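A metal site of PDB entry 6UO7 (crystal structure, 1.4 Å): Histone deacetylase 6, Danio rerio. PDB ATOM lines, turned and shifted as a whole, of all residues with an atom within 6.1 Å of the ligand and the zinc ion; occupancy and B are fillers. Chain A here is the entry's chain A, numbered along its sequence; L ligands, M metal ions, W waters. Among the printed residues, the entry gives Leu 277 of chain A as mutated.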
ATOM      1  N   ASP A  26     -18.188 -18.876 -25.759  1.00  0.00           N
ATOM      2  CA  ASP A  26     -19.565 -19.316 -25.561  1.00  0.00           C
ATOM      3  C   ASP A  26     -20.231 -18.348 -24.583  1.00  0.00           C
ATOM      4  O   ASP A  26     -20.093 -18.502 -23.370  1.00  0.00           O
ATOM      5  CB  ASP A  26     -19.632 -20.746 -25.051  1.00  0.00           C
ATOM      6  CG  ASP A  26     -21.056 -21.202 -24.762  1.00  0.00           C
ATOM      7  OD1 ASP A  26     -22.008 -20.473 -25.103  1.00  0.00           O
ATOM      8  OD2 ASP A  26     -21.228 -22.306 -24.196  1.00  0.00           O
ATOM      9  N   SER A  28     -23.195 -18.133 -23.699  1.00  0.00           N
ATOM     10  CA  SER A  28     -24.235 -18.767 -22.889  1.00  0.00           C
ATOM     11  C   SER A  28     -23.684 -19.764 -21.887  1.00  0.00           C
ATOM     12  O   SER A  28     -24.453 -20.504 -21.270  1.00  0.00           O
ATOM     13  CB  SER A  28     -25.268 -19.448 -23.782  1.00  0.00           C
ATOM     14  OG  SER A  28     -25.889 -18.516 -24.653  1.00  0.00           O
ATOM     15  N   HIS A  29     -22.366 -19.823 -21.722  1.00  0.00           N
ATOM     16  CA  HIS A  29     -21.789 -20.797 -20.809  1.00  0.00           C
ATOM     17  C   HIS A  29     -22.367 -20.606 -19.418  1.00  0.00           C
ATOM     18  O   HIS A  29     -22.453 -19.469 -18.932  1.00  0.00           O
ATOM     19  CB  HIS A  29     -20.271 -20.660 -20.752  1.00  0.00           C
ATOM     20  CG  HIS A  29     -19.594 -21.867 -20.158  1.00  0.00           C
ATOM     21  ND1 HIS A  29     -19.656 -22.162 -18.810  1.00  0.00           N
ATOM     22  CD2 HIS A  29     -18.875 -22.849 -20.734  1.00  0.00           C
ATOM     23  CE1 HIS A  29     -18.994 -23.283 -18.587  1.00  0.00           C
ATOM     24  NE2 HIS A  29     -18.507 -23.716 -19.734  1.00  0.00           N
ATOM     25  N   PRO A  30     -22.776 -21.680 -18.736  1.00  0.00           N
ATOM     26  CA  PRO A  30     -23.451 -21.517 -17.443  1.00  0.00           C
ATOM     27  C   PRO A  30     -22.533 -21.056 -16.319  1.00  0.00           C
ATOM     28  O   PRO A  30     -23.016 -20.459 -15.351  1.00  0.00           O
ATOM     29  CB  PRO A  30     -24.021 -22.912 -17.167  1.00  0.00           C
ATOM     30  CG  PRO A  30     -23.118 -23.841 -17.915  1.00  0.00           C
ATOM     31  CD  PRO A  30     -22.787 -23.090 -19.187  1.00  0.00           C
ATOM     32  N   SER A  97     -15.011 -30.820 -20.483  1.00  0.00           N
ATOM     33  CA  SER A  97     -15.956 -29.821 -19.974  1.00  0.00           C
ATOM     34  C   SER A  97     -15.259 -28.701 -19.199  1.00  0.00           C
ATOM     35  O   SER A  97     -15.600 -28.413 -18.052  1.00  0.00           O
ATOM     36  CB  SER A  97     -17.051 -30.493 -19.141  1.00  0.00           C
ATOM     37  OG  SER A  97     -17.983 -29.513 -18.701  1.00  0.00           O
ATOM     38  N   VAL A  98     -14.295 -28.037 -19.839  1.00  0.00           N
ATOM     39  CA  VAL A  98     -13.682 -26.841 -19.277  1.00  0.00           C
ATOM     40  C   VAL A  98     -13.491 -25.793 -20.354  1.00  0.00           C
ATOM     41  O   VAL A  98     -13.370 -26.101 -21.548  1.00  0.00           O
ATOM     42  CB  VAL A  98     -12.321 -27.096 -18.578  1.00  0.00           C
ATOM     43  CG1 VAL A  98     -12.442 -28.200 -17.554  1.00  0.00           C
ATOM     44  CG2 VAL A  98     -11.253 -27.434 -19.590  1.00  0.00           C
ATOM     45  N   PRO A 137     -15.047 -23.262  -9.419  1.00  0.00           N
ATOM     46  CA  PRO A 137     -15.285 -24.390  -8.511  1.00  0.00           C
ATOM     47  C   PRO A 137     -14.095 -25.338  -8.524  1.00  0.00           C
ATOM     48  O   PRO A 137     -13.149 -25.174  -9.309  1.00  0.00           O
ATOM     49  CB  PRO A 137     -16.527 -25.038  -9.120  1.00  0.00           C
ATOM     50  CG  PRO A 137     -16.389 -24.777 -10.588  1.00  0.00           C
ATOM     51  CD  PRO A 137     -15.865 -23.347 -10.630  1.00  0.00           C
ATOM     52  N   HIS A 139     -14.382 -29.229  -7.219  1.00  0.00           N
ATOM     53  CA  HIS A 139     -14.464 -30.631  -6.804  1.00  0.00           C
ATOM     54  C   HIS A 139     -14.156 -31.638  -7.911  1.00  0.00           C
ATOM     55  O   HIS A 139     -13.891 -32.811  -7.600  1.00  0.00           O
ATOM     56  CB  HIS A 139     -15.757 -30.962  -6.042  1.00  0.00           C
ATOM     57  CG  HIS A 139     -17.008 -30.877  -6.852  1.00  0.00           C
ATOM     58  ND1 HIS A 139     -18.119 -31.636  -6.548  1.00  0.00           N
ATOM     59  CD2 HIS A 139     -17.347 -30.118  -7.929  1.00  0.00           C
ATOM     60  CE1 HIS A 139     -19.076 -31.368  -7.411  1.00  0.00           C
ATOM     61  NE2 HIS A 139     -18.644 -30.431  -8.252  1.00  0.00           N
ATOM     62  N   HIS A 140     -14.203 -31.238  -9.179  1.00  0.00           N
ATOM     63  CA  HIS A 140     -13.831 -32.145 -10.269  1.00  0.00           C
ATOM     64  C   HIS A 140     -12.347 -32.106 -10.618  1.00  0.00           C
ATOM     65  O   HIS A 140     -11.886 -33.002 -11.332  1.00  0.00           O
ATOM     66  CB  HIS A 140     -14.608 -31.801 -11.537  1.00  0.00           C
ATOM     67  CG  HIS A 140     -16.088 -31.926 -11.383  1.00  0.00           C
ATOM     68  ND1 HIS A 140     -16.704 -33.102 -11.016  1.00  0.00           N
ATOM     69  CD2 HIS A 140     -17.080 -31.015 -11.518  1.00  0.00           C
ATOM     70  CE1 HIS A 140     -18.001 -32.915 -10.942  1.00  0.00           C
ATOM     71  NE2 HIS A 140     -18.261 -31.658 -11.248  1.00  0.00           N
ATOM     72  N   GLY A 148     -14.540 -30.396 -15.675  1.00  0.00           N
ATOM     73  CA  GLY A 148     -15.828 -29.960 -15.146  1.00  0.00           C
ATOM     74  C   GLY A 148     -15.836 -28.562 -14.571  1.00  0.00           C
ATOM     75  O   GLY A 148     -16.339 -28.334 -13.456  1.00  0.00           O
ATOM     76  N   PHE A 149     -15.264 -27.612 -15.312  1.00  0.00           N
ATOM     77  CA  PHE A 149     -15.226 -26.190 -14.984  1.00  0.00           C
ATOM     78  C   PHE A 149     -14.213 -25.875 -13.890  1.00  0.00           C
ATOM     79  O   PHE A 149     -14.168 -24.733 -13.419  1.00  0.00           O
ATOM     80  CB  PHE A 149     -16.582 -25.588 -14.577  1.00  0.00           C
ATOM     81  CG  PHE A 149     -17.715 -25.848 -15.543  1.00  0.00           C
ATOM     82  CD1 PHE A 149     -19.033 -25.784 -15.097  1.00  0.00           C
ATOM     83  CD2 PHE A 149     -17.491 -26.167 -16.882  1.00  0.00           C
ATOM     84  CE1 PHE A 149     -20.102 -26.005 -15.950  1.00  0.00           C
ATOM     85  CE2 PHE A 149     -18.557 -26.404 -17.750  1.00  0.00           C
ATOM     86  CZ  PHE A 149     -19.868 -26.326 -17.279  1.00  0.00           C
ATOM     87  N   CYS A 150     -13.392 -26.849 -13.482  1.00  0.00           N
ATOM     88  CA  CYS A 150     -12.499 -26.729 -12.338  1.00  0.00           C
ATOM     89  C   CYS A 150     -11.043 -26.835 -12.783  1.00  0.00           C
ATOM     90  O   CYS A 150     -10.702 -27.669 -13.618  1.00  0.00           O
ATOM     91  CB  CYS A 150     -12.727 -27.858 -11.325  1.00  0.00           C
ATOM     92  SG  CYS A 150     -14.400 -27.972 -10.675  1.00  0.00           S
ATOM     93  N   ASP A 177     -23.317 -30.834  -4.010  1.00  0.00           N
ATOM     94  CA  ASP A 177     -23.490 -30.470  -5.397  1.00  0.00           C
ATOM     95  C   ASP A 177     -24.159 -31.639  -6.137  1.00  0.00           C
ATOM     96  O   ASP A 177     -23.986 -32.804  -5.766  1.00  0.00           O
ATOM     97  CB  ASP A 177     -22.101 -30.171  -5.975  1.00  0.00           C
ATOM     98  CG  ASP A 177     -22.150 -29.633  -7.377  1.00  0.00           C
ATOM     99  OD1 ASP A 177     -22.336 -30.415  -8.347  1.00  0.00           O
ATOM    100  OD2 ASP A 177     -21.989 -28.403  -7.547  1.00  0.00           O
ATOM    101  N   VAL A 178     -24.931 -31.327  -7.174  1.00  0.00           N
ATOM    102  CA  VAL A 178     -25.671 -32.371  -7.881  1.00  0.00           C
ATOM    103  C   VAL A 178     -24.755 -33.317  -8.666  1.00  0.00           C
ATOM    104  O   VAL A 178     -25.194 -34.399  -9.066  1.00  0.00           O
ATOM    105  CB  VAL A 178     -26.757 -31.756  -8.796  1.00  0.00           C
ATOM    106  CG1 VAL A 178     -26.162 -31.312 -10.136  1.00  0.00           C
ATOM    107  CG2 VAL A 178     -27.913 -32.732  -8.999  1.00  0.00           C
ATOM    108  N   HIS A 179     -23.513 -32.920  -8.901  1.00  0.00           N
ATOM    109  CA  HIS A 179     -22.554 -33.755  -9.612  1.00  0.00           C
ATOM    110  C   HIS A 179     -21.644 -34.475  -8.626  1.00  0.00           C
ATOM    111  O   HIS A 179     -21.377 -33.998  -7.525  1.00  0.00           O
ATOM    112  CB  HIS A 179     -21.685 -32.891 -10.530  1.00  0.00           C
ATOM    113  CG  HIS A 179     -22.451 -32.187 -11.592  1.00  0.00           C
ATOM    114  ND1 HIS A 179     -22.908 -30.892 -11.456  1.00  0.00           N
ATOM    115  CD2 HIS A 179     -22.851 -32.592 -12.820  1.00  0.00           C
ATOM    116  CE1 HIS A 179     -23.557 -30.531 -12.547  1.00  0.00           C
ATOM    117  NE2 HIS A 179     -23.532 -31.543 -13.390  1.00  0.00           N
ATOM    118  N   TRP A 208     -23.746 -36.697 -16.617  1.00  0.00           N
ATOM    119  CA  TRP A 208     -22.333 -36.350 -16.541  1.00  0.00           C
ATOM    120  C   TRP A 208     -21.861 -36.381 -15.076  1.00  0.00           C
ATOM    121  O   TRP A 208     -22.596 -35.916 -14.188  1.00  0.00           O
ATOM    122  CB  TRP A 208     -22.140 -34.945 -17.140  1.00  0.00           C
ATOM    123  CG  TRP A 208     -20.707 -34.605 -17.361  1.00  0.00           C
ATOM    124  CD1 TRP A 208     -19.992 -34.763 -18.518  1.00  0.00           C
ATOM    125  CD2 TRP A 208     -19.793 -34.061 -16.399  1.00  0.00           C
ATOM    126  NE1 TRP A 208     -18.692 -34.353 -18.332  1.00  0.00           N
ATOM    127  CE2 TRP A 208     -18.540 -33.915 -17.038  1.00  0.00           C
ATOM    128  CE3 TRP A 208     -19.907 -33.673 -15.055  1.00  0.00           C
ATOM    129  CZ2 TRP A 208     -17.416 -33.418 -16.386  1.00  0.00           C
ATOM    130  CZ3 TRP A 208     -18.790 -33.187 -14.405  1.00  0.00           C
ATOM    131  CH2 TRP A 208     -17.564 -33.070 -15.063  1.00  0.00           C
ATOM    132  N   HIS A 210     -20.677 -39.494 -15.997  1.00  0.00           N
ATOM    133  CA  HIS A 210     -20.866 -40.808 -16.639  1.00  0.00           C
ATOM    134  C   HIS A 210     -19.897 -41.878 -16.154  1.00  0.00           C
ATOM    135  O   HIS A 210     -19.493 -42.733 -16.957  1.00  0.00           O
ATOM    136  CB  HIS A 210     -20.733 -40.699 -18.165  1.00  0.00           C
ATOM    137  CG  HIS A 210     -21.472 -39.542 -18.771  1.00  0.00           C
ATOM    138  ND1 HIS A 210     -22.842 -39.474 -18.825  1.00  0.00           N
ATOM    139  CD2 HIS A 210     -21.019 -38.421 -19.378  1.00  0.00           C
ATOM    140  CE1 HIS A 210     -23.210 -38.355 -19.420  1.00  0.00           C
ATOM    141  NE2 HIS A 210     -22.113 -37.697 -19.776  1.00  0.00           N
ATOM    142  N   GLY A 268     -22.343 -26.857  -3.708  1.00  0.00           N
ATOM    143  CA  GLY A 268     -22.987 -26.530  -4.957  1.00  0.00           C
ATOM    144  C   GLY A 268     -24.484 -26.422  -4.771  1.00  0.00           C
ATOM    145  O   GLY A 268     -25.055 -27.013  -3.856  1.00  0.00           O
ATOM    146  N   ASP A 270     -26.701 -26.696  -7.604  1.00  0.00           N
ATOM    147  CA  ASP A 270     -27.336 -27.153  -8.826  1.00  0.00           C
ATOM    148  C   ASP A 270     -28.384 -28.230  -8.594  1.00  0.00           C
ATOM    149  O   ASP A 270     -29.049 -28.627  -9.554  1.00  0.00           O
ATOM    150  CB  ASP A 270     -26.312 -27.525  -9.919  1.00  0.00           C
ATOM    151  CG  ASP A 270     -25.095 -28.261  -9.385  1.00  0.00           C
ATOM    152  OD1 ASP A 270     -25.127 -28.740  -8.243  1.00  0.00           O
ATOM    153  OD2 ASP A 270     -24.089 -28.343 -10.135  1.00  0.00           O
ATOM    154  N   LEU A 277     -29.588 -27.360 -15.224  1.00  0.00           N
ATOM    155  CA  LEU A 277     -28.875 -28.605 -15.515  1.00  0.00           C
ATOM    156  C   LEU A 277     -29.134 -29.726 -14.509  1.00  0.00           C
ATOM    157  O   LEU A 277     -29.073 -30.898 -14.869  1.00  0.00           O
ATOM    158  CB  LEU A 277     -27.353 -28.372 -15.459  1.00  0.00           C
ATOM    159  CG  LEU A 277     -26.723 -27.280 -16.315  1.00  0.00           C
ATOM    160  CD1 LEU A 277     -25.231 -27.170 -16.055  1.00  0.00           C
ATOM    161  CD2 LEU A 277     -27.002 -27.559 -17.773  1.00  0.00           C
ATOM    162  N   GLU A 307     -19.435 -24.531  -5.116  1.00  0.00           N
ATOM    163  CA  GLU A 307     -19.084 -25.371  -6.257  1.00  0.00           C
ATOM    164  C   GLU A 307     -19.979 -24.933  -7.416  1.00  0.00           C
ATOM    165  O   GLU A 307     -19.831 -23.810  -7.891  1.00  0.00           O
ATOM    166  CB  GLU A 307     -19.192 -26.864  -5.901  1.00  0.00           C
ATOM    167  CG  GLU A 307     -18.218 -27.293  -4.796  1.00  0.00           C
ATOM    168  CD  GLU A 307     -16.773 -27.451  -5.247  1.00  0.00           C
ATOM    169  OE1 GLU A 307     -15.927 -27.722  -4.368  1.00  0.00           O
ATOM    170  OE2 GLU A 307     -16.463 -27.309  -6.456  1.00  0.00           O
ATOM    171  N   GLY A 308     -20.912 -25.787  -7.855  1.00  0.00           N
ATOM    172  CA  GLY A 308     -21.810 -25.448  -8.939  1.00  0.00           C
ATOM    173  C   GLY A 308     -23.088 -24.768  -8.471  1.00  0.00           C
ATOM    174  O   GLY A 308     -23.225 -24.303  -7.342  1.00  0.00           O
ATOM    175  N   GLY A 309     -24.052 -24.704  -9.396  1.00  0.00           N
ATOM    176  CA  GLY A 309     -25.297 -23.984  -9.200  1.00  0.00           C
ATOM    177  C   GLY A 309     -25.396 -22.900 -10.241  1.00  0.00           C
ATOM    178  O   GLY A 309     -24.600 -21.954 -10.228  1.00  0.00           O
ATOM    179  N   TYR A 310     -26.384 -22.996 -11.142  1.00  0.00           N
ATOM    180  CA  TYR A 310     -26.382 -22.216 -12.377  1.00  0.00           C
ATOM    181  C   TYR A 310     -27.633 -21.398 -12.622  1.00  0.00           C
ATOM    182  O   TYR A 310     -27.652 -20.613 -13.582  1.00  0.00           O
ATOM    183  CB  TYR A 310     -26.070 -23.128 -13.581  1.00  0.00           C
ATOM    184  CG  TYR A 310     -24.759 -23.821 -13.332  1.00  0.00           C
ATOM    185  CD1 TYR A 310     -23.568 -23.118 -13.416  1.00  0.00           C
ATOM    186  CD2 TYR A 310     -24.715 -25.127 -12.883  1.00  0.00           C
ATOM    187  CE1 TYR A 310     -22.344 -23.716 -13.111  1.00  0.00           C
ATOM    188  CE2 TYR A 310     -23.520 -25.733 -12.569  1.00  0.00           C
ATOM    189  CZ  TYR A 310     -22.339 -25.027 -12.704  1.00  0.00           C
ATOM    190  OH  TYR A 310     -21.135 -25.627 -12.399  1.00  0.00           O
HETATM  191  C1  LIG L   1     -22.280 -30.815 -20.928  1.00  0.00           C
HETATM  192  C2  LIG L   1     -21.388 -28.424 -20.594  1.00  0.00           C
HETATM  193  C3  LIG L   1     -22.569 -26.310 -20.930  1.00  0.00           C
HETATM  194  C4  LIG L   1     -20.256 -26.451 -21.453  1.00  0.00           C
HETATM  195  C5  LIG L   1     -21.745 -28.874 -15.743  1.00  0.00           C
HETATM  196  C6  LIG L   1     -21.764 -28.633 -14.387  1.00  0.00           C
HETATM  197  C7  LIG L   1     -20.837 -28.834 -12.128  1.00  0.00           C
HETATM  198  C8  LIG L   1     -20.734 -29.037 -13.560  1.00  0.00           C
HETATM  199  C9  LIG L   1     -19.688 -29.726 -14.188  1.00  0.00           C
HETATM  200  C10 LIG L   1     -19.669 -29.964 -15.554  1.00  0.00           C
HETATM  201  C11 LIG L   1     -20.698 -29.569 -16.383  1.00  0.00           C
HETATM  202  C12 LIG L   1     -21.707 -29.856 -18.655  1.00  0.00           C
HETATM  203  C13 LIG L   1     -21.377 -29.894 -20.121  1.00  0.00           C
HETATM  204  C14 LIG L   1     -22.171 -32.267 -20.455  1.00  0.00           C
HETATM  205  C15 LIG L   1     -21.940 -30.790 -22.418  1.00  0.00           C
HETATM  206  C16 LIG L   1     -22.540 -27.646 -20.532  1.00  0.00           C
HETATM  207  C17 LIG L   1     -21.423 -25.704 -21.399  1.00  0.00           C
HETATM  208  C18 LIG L   1     -20.238 -27.779 -21.051  1.00  0.00           C
HETATM  209  N1  LIG L   1     -20.682 -29.734 -17.715  1.00  0.00           N
HETATM  210  N2  LIG L   1     -20.124 -29.710 -11.285  1.00  0.00           N
HETATM  211  O1  LIG L   1     -21.603 -28.062 -11.615  1.00  0.00           O
HETATM  212  O2  LIG L   1     -22.876 -29.896 -18.270  1.00  0.00           O
HETATM  213  O3  LIG L   1     -20.219 -29.617  -9.939  1.00  0.00           O
HETATM  214 ZN    ZN M   1     -22.319 -29.360 -10.064  1.00  0.00          ZN
HETATM  215  O   HOH W   1     -25.656 -25.109 -20.004  1.00  0.00           O
HETATM  216  O   HOH W   2     -17.201 -27.885 -22.733  1.00  0.00           O
HETATM  217  O   HOH W   3     -25.366 -30.166 -19.440  1.00  0.00           O
HETATM  218  O   HOH W   4     -24.214 -31.417 -16.115  1.00  0.00           O
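An oxygen (O3) of the ligand lies close to a ring nitrogen (NE2) of His 139 (2.4 Å).
OH of Tyr 310 lies close to O1 of the ligand (2.6 Å).
N2 of the ligand lies close to NE2 of His 140.
OG of Ser 97 lies within hydrogen-bond range of N1 of the ligand, at 2.9 Å.
The backbone NH of Gly 308 is in hydrogen-bond range of the side-chain carboxylate of Asp 177.
The side-chain carboxylate (OD1) of Asp 270 is in hydrogen-bond range of the backbone NH (N) of Val 178 (2.8 Å).
N of His 139 is in hydrogen-bond range of OE2 of Glu 307 (2.9 Å).
The backbone NH (N) of His 139 lies within hydrogen-bond range of the side-chain sulfur (SG) of Cys 150.
The side-chain sulfur of Cys 150 sits at hydrogen-bond distance from the backbone NH of His 140, at 3.6 Å.
The backbone carbonyl oxygen (O) of Ser 97 sits at hydrogen-bond distance from the backbone NH (N) of Phe 149 (2.9 Å).
O of Ser 97 lies within hydrogen-bond range of N of Gly 148, 3.3 Å away.
N of His 29 sits at hydrogen-bond distance from OD1 of Asp 26, 3.5 Å away.
His 29 touches the ligand (NE2 to C4, 3.7 Å).
Pro 30 touches the ligand (CD to C3, 3.7 Å).
O of Gly 148 touches C9 of the ligand, 3.7 Å away.
CE1 of Phe 149 touches C5 of the ligand, 3.3 Å away.
CZ3 of Trp 208 touches C10 of the ligand, 3.5 Å away.
CD1 of Leu 277 touches C5 of the ligand (3.9 Å).
Gly 308 touches the ligand (CA to O1, 3.7 Å).
Hydrophobic or aromatic side chains that line the ligand: His 29, Pro 30, His 139, His 140, Phe 149, His 179, Trp 208, Leu 277 and Tyr 310.
Within 4 Å of the ligand: His 29, Pro 30, Ser 97, His 139, His 140, Gly 148, Phe 149, Asp 177, His 179, Trp 208, Asp 270, Leu 277, Gly 308 and Tyr 310.
The nearest printed residue that does not touch the ligand is Asp 26 (4.4 Å).
Within 4 Å of the zinc ion: Asp 177, His 179 and Asp 270.
The zinc ion is bound by OD1 of Asp 177 (2.0 Å), OD2 of Asp 270 (2.0 Å), O3 of the ligand (2.1 Å), O1 of the ligand (2.1 Å) and ND1 of His 179 (2.2 Å).
The zinc ion has five donor atoms within binding distance.
Slightly farther from the zinc ion lies the side-chain carboxylate (OD2) of Asp 177 (2.7 Å).
Water W4 bridges a ring nitrogen (NE2) of His 179 and an oxygen (O2) of the ligand.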
